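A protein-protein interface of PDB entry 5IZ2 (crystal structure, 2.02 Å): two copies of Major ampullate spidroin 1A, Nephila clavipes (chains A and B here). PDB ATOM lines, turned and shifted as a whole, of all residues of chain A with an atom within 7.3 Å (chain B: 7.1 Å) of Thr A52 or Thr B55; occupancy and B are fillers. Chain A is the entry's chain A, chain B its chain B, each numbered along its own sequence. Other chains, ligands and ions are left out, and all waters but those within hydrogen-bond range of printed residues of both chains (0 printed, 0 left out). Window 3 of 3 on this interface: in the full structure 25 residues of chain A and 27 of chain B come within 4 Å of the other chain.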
ATOM      1  N   ILE A  25      -0.071 -10.337 -20.229  1.00  0.00           N
ATOM      2  CA  ILE A  25       1.131  -9.762 -19.637  1.00  0.00           C
ATOM      3  C   ILE A  25       1.648 -10.639 -18.489  1.00  0.00           C
ATOM      4  O   ILE A  25       2.845 -10.927 -18.416  1.00  0.00           O
ATOM      5  CB  ILE A  25       0.868  -8.311 -19.162  1.00  0.00           C
ATOM      6  CG1 ILE A  25       0.818  -7.388 -20.391  1.00  0.00           C
ATOM      7  CG2 ILE A  25       1.952  -7.839 -18.197  1.00  0.00           C
ATOM      8  CD1 ILE A  25       0.282  -5.995 -20.118  1.00  0.00           C
ATOM      9  N   MET A  46      11.221  -5.385 -17.074  1.00  0.00           N
ATOM     10  CA  MET A  46      10.067  -5.940 -17.770  1.00  0.00           C
ATOM     11  C   MET A  46       8.848  -5.935 -16.861  1.00  0.00           C
ATOM     12  O   MET A  46       7.741  -5.593 -17.290  1.00  0.00           O
ATOM     13  CB  MET A  46      10.354  -7.360 -18.248  1.00  0.00           C
ATOM     14  CG  MET A  46      11.427  -7.445 -19.313  1.00  0.00           C
ATOM     15  SD  MET A  46      11.803  -9.158 -19.729  1.00  0.00           S
ATOM     16  CE  MET A  46      13.066  -8.927 -20.977  1.00  0.00           C
ATOM     17  N   SER A  47       9.061  -6.330 -15.609  1.00  0.00           N
ATOM     18  CA  SER A  47       7.992  -6.378 -14.626  1.00  0.00           C
ATOM     19  C   SER A  47       7.418  -4.986 -14.351  1.00  0.00           C
ATOM     20  O   SER A  47       6.203  -4.819 -14.237  1.00  0.00           O
ATOM     21  CB  SER A  47       8.497  -7.015 -13.326  1.00  0.00           C
ATOM     22  OG  SER A  47       7.463  -7.092 -12.357  1.00  0.00           O
ATOM     23  N   THR A  48       8.291  -3.991 -14.248  1.00  0.00           N
ATOM     24  CA  THR A  48       7.844  -2.625 -13.991  1.00  0.00           C
ATOM     25  C   THR A  48       6.978  -2.095 -15.132  1.00  0.00           C
ATOM     26  O   THR A  48       5.888  -1.566 -14.907  1.00  0.00           O
ATOM     27  CB  THR A  48       9.034  -1.674 -13.781  1.00  0.00           C
ATOM     28  OG1 THR A  48       9.717  -2.028 -12.575  1.00  0.00           O
ATOM     29  CG2 THR A  48       8.553  -0.227 -13.677  1.00  0.00           C
ATOM     30  N   ILE A  49       7.460  -2.267 -16.357  1.00  0.00           N
ATOM     31  CA  ILE A  49       6.717  -1.853 -17.541  1.00  0.00           C
ATOM     32  C   ILE A  49       5.397  -2.616 -17.652  1.00  0.00           C
ATOM     33  O   ILE A  49       4.356  -2.034 -17.952  1.00  0.00           O
ATOM     34  CB  ILE A  49       7.571  -2.036 -18.804  1.00  0.00           C
ATOM     35  CG1 ILE A  49       8.768  -1.081 -18.728  1.00  0.00           C
ATOM     36  CG2 ILE A  49       6.748  -1.749 -20.053  1.00  0.00           C
ATOM     37  CD1 ILE A  49       9.953  -1.480 -19.568  1.00  0.00           C
ATOM     38  N   GLY A  50       5.439  -3.920 -17.410  1.00  0.00           N
ATOM     39  CA  GLY A  50       4.229  -4.714 -17.435  1.00  0.00           C
ATOM     40  C   GLY A  50       3.228  -4.222 -16.402  1.00  0.00           C
ATOM     41  O   GLY A  50       2.049  -4.074 -16.700  1.00  0.00           O
ATOM     42  N   ASP A  51       3.705  -3.972 -15.184  1.00  0.00           N
ATOM     43  CA  ASP A  51       2.858  -3.477 -14.099  1.00  0.00           C
ATOM     44  C   ASP A  51       2.233  -2.129 -14.435  1.00  0.00           C
ATOM     45  O   ASP A  51       1.071  -1.878 -14.113  1.00  0.00           O
ATOM     46  CB  ASP A  51       3.654  -3.350 -12.797  1.00  0.00           C
ATOM     47  CG  ASP A  51       2.799  -2.858 -11.634  1.00  0.00           C
ATOM     48  OD1 ASP A  51       2.021  -3.666 -11.077  1.00  0.00           O
ATOM     49  OD2 ASP A  51       2.896  -1.656 -11.288  1.00  0.00           O
ATOM     50  N   THR A  52       3.015  -1.256 -15.060  1.00  0.00           N
ATOM     51  CA  THR A  52       2.515   0.060 -15.441  1.00  0.00           C
ATOM     52  C   THR A  52       1.387  -0.044 -16.453  1.00  0.00           C
ATOM     53  O   THR A  52       0.366   0.628 -16.321  1.00  0.00           O
ATOM     54  CB  THR A  52       3.637   0.934 -16.033  1.00  0.00           C
ATOM     55  OG1 THR A  52       4.674   1.095 -15.059  1.00  0.00           O
ATOM     56  CG2 THR A  52       3.118   2.311 -16.415  1.00  0.00           C
ATOM     57  N   ILE A  53       1.565  -0.900 -17.455  1.00  0.00           N
ATOM     58  CA  ILE A  53       0.554  -1.056 -18.497  1.00  0.00           C
ATOM     59  C   ILE A  53      -0.728  -1.691 -17.939  1.00  0.00           C
ATOM     60  O   ILE A  53      -1.830  -1.203 -18.197  1.00  0.00           O
ATOM     61  CB  ILE A  53       1.118  -1.875 -19.684  1.00  0.00           C
ATOM     62  CG1 ILE A  53       2.196  -1.042 -20.407  1.00  0.00           C
ATOM     63  CG2 ILE A  53       0.007  -2.280 -20.665  1.00  0.00           C
ATOM     64  CD1 ILE A  53       2.971  -1.802 -21.461  1.00  0.00           C
ATOM     65  N   LYS A  54      -0.581  -2.747 -17.141  1.00  0.00           N
ATOM     66  CA  LYS A  54      -1.740  -3.391 -16.537  1.00  0.00           C
ATOM     67  C   LYS A  54      -2.547  -2.414 -15.686  1.00  0.00           C
ATOM     68  O   LYS A  54      -3.767  -2.360 -15.785  1.00  0.00           O
ATOM     69  CB  LYS A  54      -1.310  -4.573 -15.666  1.00  0.00           C
ATOM     70  CG  LYS A  54      -0.847  -5.805 -16.434  1.00  0.00           C
ATOM     71  CD  LYS A  54      -0.679  -6.975 -15.479  1.00  0.00           C
ATOM     72  CE  LYS A  54       0.480  -6.751 -14.522  1.00  0.00           C
ATOM     73  NZ  LYS A  54       0.469  -7.737 -13.400  1.00  0.00           N
ATOM     74  N   THR A  55      -1.851  -1.616 -14.885  1.00  0.00           N
ATOM     75  CA  THR A  55      -2.503  -0.634 -14.022  1.00  0.00           C
ATOM     76  C   THR A  55      -3.271   0.394 -14.837  1.00  0.00           C
ATOM     77  O   THR A  55      -4.404   0.748 -14.496  1.00  0.00           O
ATOM     78  CB  THR A  55      -1.481   0.069 -13.108  1.00  0.00           C
ATOM     79  OG1 THR A  55      -0.939  -0.897 -12.200  1.00  0.00           O
ATOM     80  CG2 THR A  55      -2.144   1.184 -12.299  1.00  0.00           C
ATOM     81  N   ALA A  56      -2.658   0.863 -15.917  1.00  0.00           N
ATOM     82  CA  ALA A  56      -3.318   1.811 -16.802  1.00  0.00           C
ATOM     83  C   ALA A  56      -4.583   1.194 -17.376  1.00  0.00           C
ATOM     84  O   ALA A  56      -5.631   1.834 -17.393  1.00  0.00           O
ATOM     85  CB  ALA A  56      -2.379   2.253 -17.929  1.00  0.00           C
ATOM     86  N   MET A  57      -4.484  -0.048 -17.850  1.00  0.00           N
ATOM     87  CA  MET A  57      -5.650  -0.744 -18.380  1.00  0.00           C
ATOM     88  C   MET A  57      -6.748  -0.970 -17.342  1.00  0.00           C
ATOM     89  O   MET A  57      -7.929  -0.830 -17.651  1.00  0.00           O
ATOM     90  CB  MET A  57      -5.259  -2.091 -18.992  1.00  0.00           C
ATOM     91  CG  MET A  57      -4.403  -1.968 -20.240  1.00  0.00           C
ATOM     92  SD  MET A  57      -4.102  -3.558 -21.030  1.00  0.00           S
ATOM     93  CE  MET A  57      -3.052  -4.367 -19.846  1.00  0.00           C
ATOM     94  N   ASP A  58      -6.359  -1.346 -16.126  1.00  0.00           N
ATOM     95  CA  ASP A  58      -7.335  -1.615 -15.069  1.00  0.00           C
ATOM     96  C   ASP A  58      -8.110  -0.343 -14.724  1.00  0.00           C
ATOM     97  O   ASP A  58      -9.333  -0.373 -14.549  1.00  0.00           O
ATOM     98  CB  ASP A  58      -6.643  -2.189 -13.821  1.00  0.00           C
ATOM     99  CG  ASP A  58      -6.024  -3.556 -14.076  1.00  0.00           C
ATOM    100  OD1 ASP A  58      -6.475  -4.238 -15.020  1.00  0.00           O
ATOM    101  OD2 ASP A  58      -5.095  -3.952 -13.335  1.00  0.00           O
ATOM    102  N   LEU A  74      -1.588  -0.937 -26.632  1.00  0.00           N
ATOM    103  CA  LEU A  74      -0.872  -1.159 -25.377  1.00  0.00           C
ATOM    104  C   LEU A  74      -0.189  -2.524 -25.398  1.00  0.00           C
ATOM    105  O   LEU A  74       0.907  -2.684 -24.868  1.00  0.00           O
ATOM    106  CB  LEU A  74      -1.821  -1.048 -24.175  1.00  0.00           C
ATOM    107  CG  LEU A  74      -2.121   0.385 -23.702  1.00  0.00           C
ATOM    108  CD1 LEU A  74      -3.280   0.400 -22.723  1.00  0.00           C
ATOM    109  CD2 LEU A  74      -0.893   1.038 -23.067  1.00  0.00           C
ATOM    110  N   ASP B  22       9.948  12.891 -21.983  1.00  0.00           N
ATOM    111  CA  ASP B  22       8.568  13.388 -21.890  1.00  0.00           C
ATOM    112  C   ASP B  22       8.283  14.408 -22.976  1.00  0.00           C
ATOM    113  O   ASP B  22       7.215  14.396 -23.600  1.00  0.00           O
ATOM    114  CB  ASP B  22       8.293  14.051 -20.538  1.00  0.00           C
ATOM    115  CG  ASP B  22       8.269  13.072 -19.383  1.00  0.00           C
ATOM    116  OD1 ASP B  22       8.125  11.846 -19.606  1.00  0.00           O
ATOM    117  OD2 ASP B  22       8.406  13.549 -18.234  1.00  0.00           O
ATOM    118  N   ILE B  49      -1.279   5.675 -25.012  1.00  0.00           N
ATOM    119  CA  ILE B  49       0.038   5.037 -25.068  1.00  0.00           C
ATOM    120  C   ILE B  49       1.135   5.961 -24.525  1.00  0.00           C
ATOM    121  O   ILE B  49       1.987   5.543 -23.729  1.00  0.00           O
ATOM    122  CB  ILE B  49       0.437   4.644 -26.508  1.00  0.00           C
ATOM    123  CG1 ILE B  49      -0.553   3.648 -27.112  1.00  0.00           C
ATOM    124  CG2 ILE B  49       1.867   4.093 -26.534  1.00  0.00           C
ATOM    125  CD1 ILE B  49      -0.708   2.404 -26.316  1.00  0.00           C
ATOM    126  N   GLY B  50       1.098   7.220 -24.951  1.00  0.00           N
ATOM    127  CA  GLY B  50       2.069   8.207 -24.512  1.00  0.00           C
ATOM    128  C   GLY B  50       2.076   8.395 -23.006  1.00  0.00           C
ATOM    129  O   GLY B  50       3.132   8.417 -22.378  1.00  0.00           O
ATOM    130  N   ASP B  51       0.887   8.519 -22.425  1.00  0.00           N
ATOM    131  CA  ASP B  51       0.754   8.682 -20.979  1.00  0.00           C
ATOM    132  C   ASP B  51       1.289   7.467 -20.208  1.00  0.00           C
ATOM    133  O   ASP B  51       1.962   7.605 -19.180  1.00  0.00           O
ATOM    134  CB  ASP B  51      -0.714   8.936 -20.614  1.00  0.00           C
ATOM    135  CG  ASP B  51      -0.909   9.177 -19.131  1.00  0.00           C
ATOM    136  OD1 ASP B  51      -0.563  10.282 -18.665  1.00  0.00           O
ATOM    137  OD2 ASP B  51      -1.419   8.276 -18.439  1.00  0.00           O
ATOM    138  N   THR B  52       0.983   6.276 -20.708  1.00  0.00           N
ATOM    139  CA  THR B  52       1.427   5.040 -20.073  1.00  0.00           C
ATOM    140  C   THR B  52       2.952   4.899 -20.137  1.00  0.00           C
ATOM    141  O   THR B  52       3.584   4.480 -19.170  1.00  0.00           O
ATOM    142  CB  THR B  52       0.766   3.821 -20.720  1.00  0.00           C
ATOM    143  OG1 THR B  52      -0.655   3.992 -20.701  1.00  0.00           O
ATOM    144  CG2 THR B  52       1.143   2.557 -19.964  1.00  0.00           C
ATOM    145  N   ILE B  53       3.536   5.239 -21.283  1.00  0.00           N
ATOM    146  CA  ILE B  53       4.987   5.162 -21.447  1.00  0.00           C
ATOM    147  C   ILE B  53       5.682   6.153 -20.520  1.00  0.00           C
ATOM    148  O   ILE B  53       6.680   5.820 -19.876  1.00  0.00           O
ATOM    149  CB  ILE B  53       5.421   5.437 -22.899  1.00  0.00           C
ATOM    150  CG1 ILE B  53       4.955   4.311 -23.828  1.00  0.00           C
ATOM    151  CG2 ILE B  53       6.934   5.581 -22.993  1.00  0.00           C
ATOM    152  CD1 ILE B  53       5.599   2.983 -23.542  1.00  0.00           C
ATOM    153  N   LYS B  54       5.164   7.377 -20.455  1.00  0.00           N
ATOM    154  CA  LYS B  54       5.732   8.384 -19.562  1.00  0.00           C
ATOM    155  C   LYS B  54       5.701   7.895 -18.116  1.00  0.00           C
ATOM    156  O   LYS B  54       6.649   8.119 -17.367  1.00  0.00           O
ATOM    157  CB  LYS B  54       5.010   9.730 -19.708  1.00  0.00           C
ATOM    158  CG  LYS B  54       5.391  10.465 -20.989  1.00  0.00           C
ATOM    159  CD  LYS B  54       4.863  11.910 -21.042  1.00  0.00           C
ATOM    160  CE  LYS B  54       3.354  11.953 -21.189  1.00  0.00           C
ATOM    161  NZ  LYS B  54       2.826  13.326 -20.970  1.00  0.00           N
ATOM    162  N   THR B  55       4.616   7.232 -17.732  1.00  0.00           N
ATOM    163  CA  THR B  55       4.494   6.691 -16.378  1.00  0.00           C
ATOM    164  C   THR B  55       5.580   5.648 -16.105  1.00  0.00           C
ATOM    165  O   THR B  55       6.208   5.663 -15.046  1.00  0.00           O
ATOM    166  CB  THR B  55       3.109   6.052 -16.144  1.00  0.00           C
ATOM    167  OG1 THR B  55       2.094   7.051 -16.285  1.00  0.00           O
ATOM    168  CG2 THR B  55       3.023   5.441 -14.745  1.00  0.00           C
ATOM    169  N   ALA B  56       5.807   4.753 -17.065  1.00  0.00           N
ATOM    170  CA  ALA B  56       6.868   3.745 -16.958  1.00  0.00           C
ATOM    171  C   ALA B  56       8.257   4.380 -16.839  1.00  0.00           C
ATOM    172  O   ALA B  56       9.067   3.977 -15.998  1.00  0.00           O
ATOM    173  CB  ALA B  56       6.822   2.803 -18.153  1.00  0.00           C
ATOM    174  N   MET B  57       8.522   5.383 -17.674  1.00  0.00           N
ATOM    175  CA  MET B  57       9.797   6.095 -17.642  1.00  0.00           C
ATOM    176  C   MET B  57      10.038   6.718 -16.276  1.00  0.00           C
ATOM    177  O   MET B  57      11.152   6.696 -15.754  1.00  0.00           O
ATOM    178  CB  MET B  57       9.822   7.182 -18.709  1.00  0.00           C
ATOM    179  CG  MET B  57       9.830   6.659 -20.120  1.00  0.00           C
ATOM    180  SD  MET B  57       9.876   8.046 -21.252  1.00  0.00           S
ATOM    181  CE  MET B  57      10.249   7.233 -22.810  1.00  0.00           C
ATOM    182  N   ASP B  58       8.981   7.278 -15.705  1.00  0.00           N
ATOM    183  CA  ASP B  58       9.061   7.918 -14.403  1.00  0.00           C
ATOM    184  C   ASP B  58       9.437   6.919 -13.305  1.00  0.00           C
ATOM    185  O   ASP B  58      10.255   7.217 -12.436  1.00  0.00           O
ATOM    186  CB  ASP B  58       7.735   8.595 -14.070  1.00  0.00           C
ATOM    187  CG  ASP B  58       7.819   9.461 -12.826  1.00  0.00           C
ATOM    188  OD1 ASP B  58       8.083  10.675 -12.958  1.00  0.00           O
ATOM    189  OD2 ASP B  58       7.626   8.923 -11.716  1.00  0.00           O
ATOM    190  N   LYS B  59       8.843   5.730 -13.350  1.00  0.00           N
ATOM    191  CA  LYS B  59       9.133   4.704 -12.353  1.00  0.00           C
ATOM    192  C   LYS B  59      10.574   4.218 -12.424  1.00  0.00           C
ATOM    193  O   LYS B  59      11.232   4.055 -11.398  1.00  0.00           O
ATOM    194  CB  LYS B  59       8.179   3.522 -12.516  1.00  0.00           C
ATOM    195  CG  LYS B  59       6.757   3.836 -12.103  1.00  0.00           C
ATOM    196  CD  LYS B  59       5.869   2.614 -12.208  1.00  0.00           C
ATOM    197  CE  LYS B  59       4.467   2.920 -11.717  1.00  0.00           C
ATOM    198  NZ  LYS B  59       3.547   1.771 -11.949  1.00  0.00           N
ATOM    199  N   MET B  60      11.061   3.987 -13.637  1.00  0.00           N
ATOM    200  CA  MET B  60      12.425   3.513 -13.831  1.00  0.00           C
ATOM    201  C   MET B  60      13.448   4.559 -13.380  1.00  0.00           C
ATOM    202  O   MET B  60      14.508   4.217 -12.851  1.00  0.00           O
ATOM    203  CB  MET B  60      12.639   3.103 -15.286  1.00  0.00           C
ATOM    204  CG  MET B  60      11.902   1.805 -15.593  1.00  0.00           C
ATOM    205  SD  MET B  60      11.714   1.399 -17.328  1.00  0.00           S
ATOM    206  CE  MET B  60      13.418   1.188 -17.788  1.00  0.00           C
ATOM    207  N   ALA B  61      13.126   5.829 -13.596  1.00  0.00           N
ATOM    208  CA  ALA B  61      13.975   6.930 -13.153  1.00  0.00           C
ATOM    209  C   ALA B  61      14.185   6.894 -11.639  1.00  0.00           C
ATOM    210  O   ALA B  61      15.274   7.187 -11.145  1.00  0.00           O
ATOM    211  CB  ALA B  61      13.376   8.262 -13.568  1.00  0.00           C
ATOM    212  N   LEU B  74      12.071   2.422 -24.258  1.00  0.00           N
ATOM    213  CA  LEU B  74      10.669   2.782 -24.047  1.00  0.00           C
ATOM    214  C   LEU B  74      10.198   3.728 -25.145  1.00  0.00           C
ATOM    215  O   LEU B  74       9.046   3.678 -25.571  1.00  0.00           O
ATOM    216  CB  LEU B  74      10.458   3.402 -22.667  1.00  0.00           C
ATOM    217  CG  LEU B  74      10.350   2.388 -21.520  1.00  0.00           C
ATOM    218  CD1 LEU B  74      10.393   3.080 -20.173  1.00  0.00           C
ATOM    219  CD2 LEU B  74       9.087   1.540 -21.655  1.00  0.00           C
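Of chain B, only Thr B52, Thr B55, Ala B56 and Lys B59 come within 4 Å of Thr A52. Of chain A, only Thr A52 comes within 4 Å of Thr B55. Printed residues of chain B within 4 Å of Thr A48: Lys B59 (3.9 Å). Printed residues of chain A within 4 Å of Thr B52: Thr A52 (3.5 Å), Ile A53 (3.8 Å), Ala A56 (3.7 Å) and Leu A74 (3.8 Å). Of the printed residues of chain B, Ile A53 touches Thr B52. Of the printed residues of chain B, Ile A49 touches Leu B74. Asp A58 touches none of the printed residues of chain B. Thr A55 touches none of the printed residues of chain B. The nearest residue of chain B that does not touch Thr A52 is Ile B53 (5.7 Å). The nearest residue of chain A that does not touch Thr B55 is Thr A48 (6.5 Å).
Of the 15 printed residues of chain B, 6 touch a printed residue of chain A. Among the printed residues, Asp or Glu carboxylates within 4 Å of a Lys or Arg side-chain nitrogen of the other chain: Asp A51 with Lys B59 (3.6 Å).
The side-chain amino group (NZ) of Lys B59 is in salt-bridge range of the side-chain carboxylate (OD2) of Asp A51 (3.6 Å). The side-chain amino group (NZ) of Lys B59 lies within hydrogen-bond range of the side-chain hydroxyl (OG1) of Thr A52 (3.4 Å).
Ile A49 touches Leu B74, and with the chains exchanged Leu A74 touches Ile B49. Thr A52 touches its own counterpart, Thr B52. Thr A52 touches Thr B55, but with the chains exchanged Thr A55 does not touch Thr B52 (7.1 Å). Ile A53 touches Thr B52, but with the chains exchanged Thr A52 does not touch Ile B53 (5.7 Å).
Among the printed residues, pairs that only touch across the chains: Leu A74 with Ile B49 (3.5 Å), Thr A52 with Thr B52 (3.5 Å), Thr A52 with Thr B55 (3.5 Å), Thr A52 with Ala B56 (3.7 Å), Ala A56 with Thr B52 (3.7 Å), Ile A49 with Leu B74 (3.8 Å), Ile A53 with Thr B52 (3.8 Å), Leu A74 with Thr B52 (3.8 Å) and Thr A48 with Lys B59 (3.9 Å).
The backbone carbonyl oxygen of Thr A48 is in hydrogen-bond range of the side-chain hydroxyl of Thr A52 (2.9 Å). O of Asp B51 lies within hydrogen-bond range of OG1 of Thr B55 (3.0 Å). The side-chain hydroxyl (OG1) of Thr A55 lies within hydrogen-bond range of the backbone carbonyl oxygen (O) of Asp A51.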
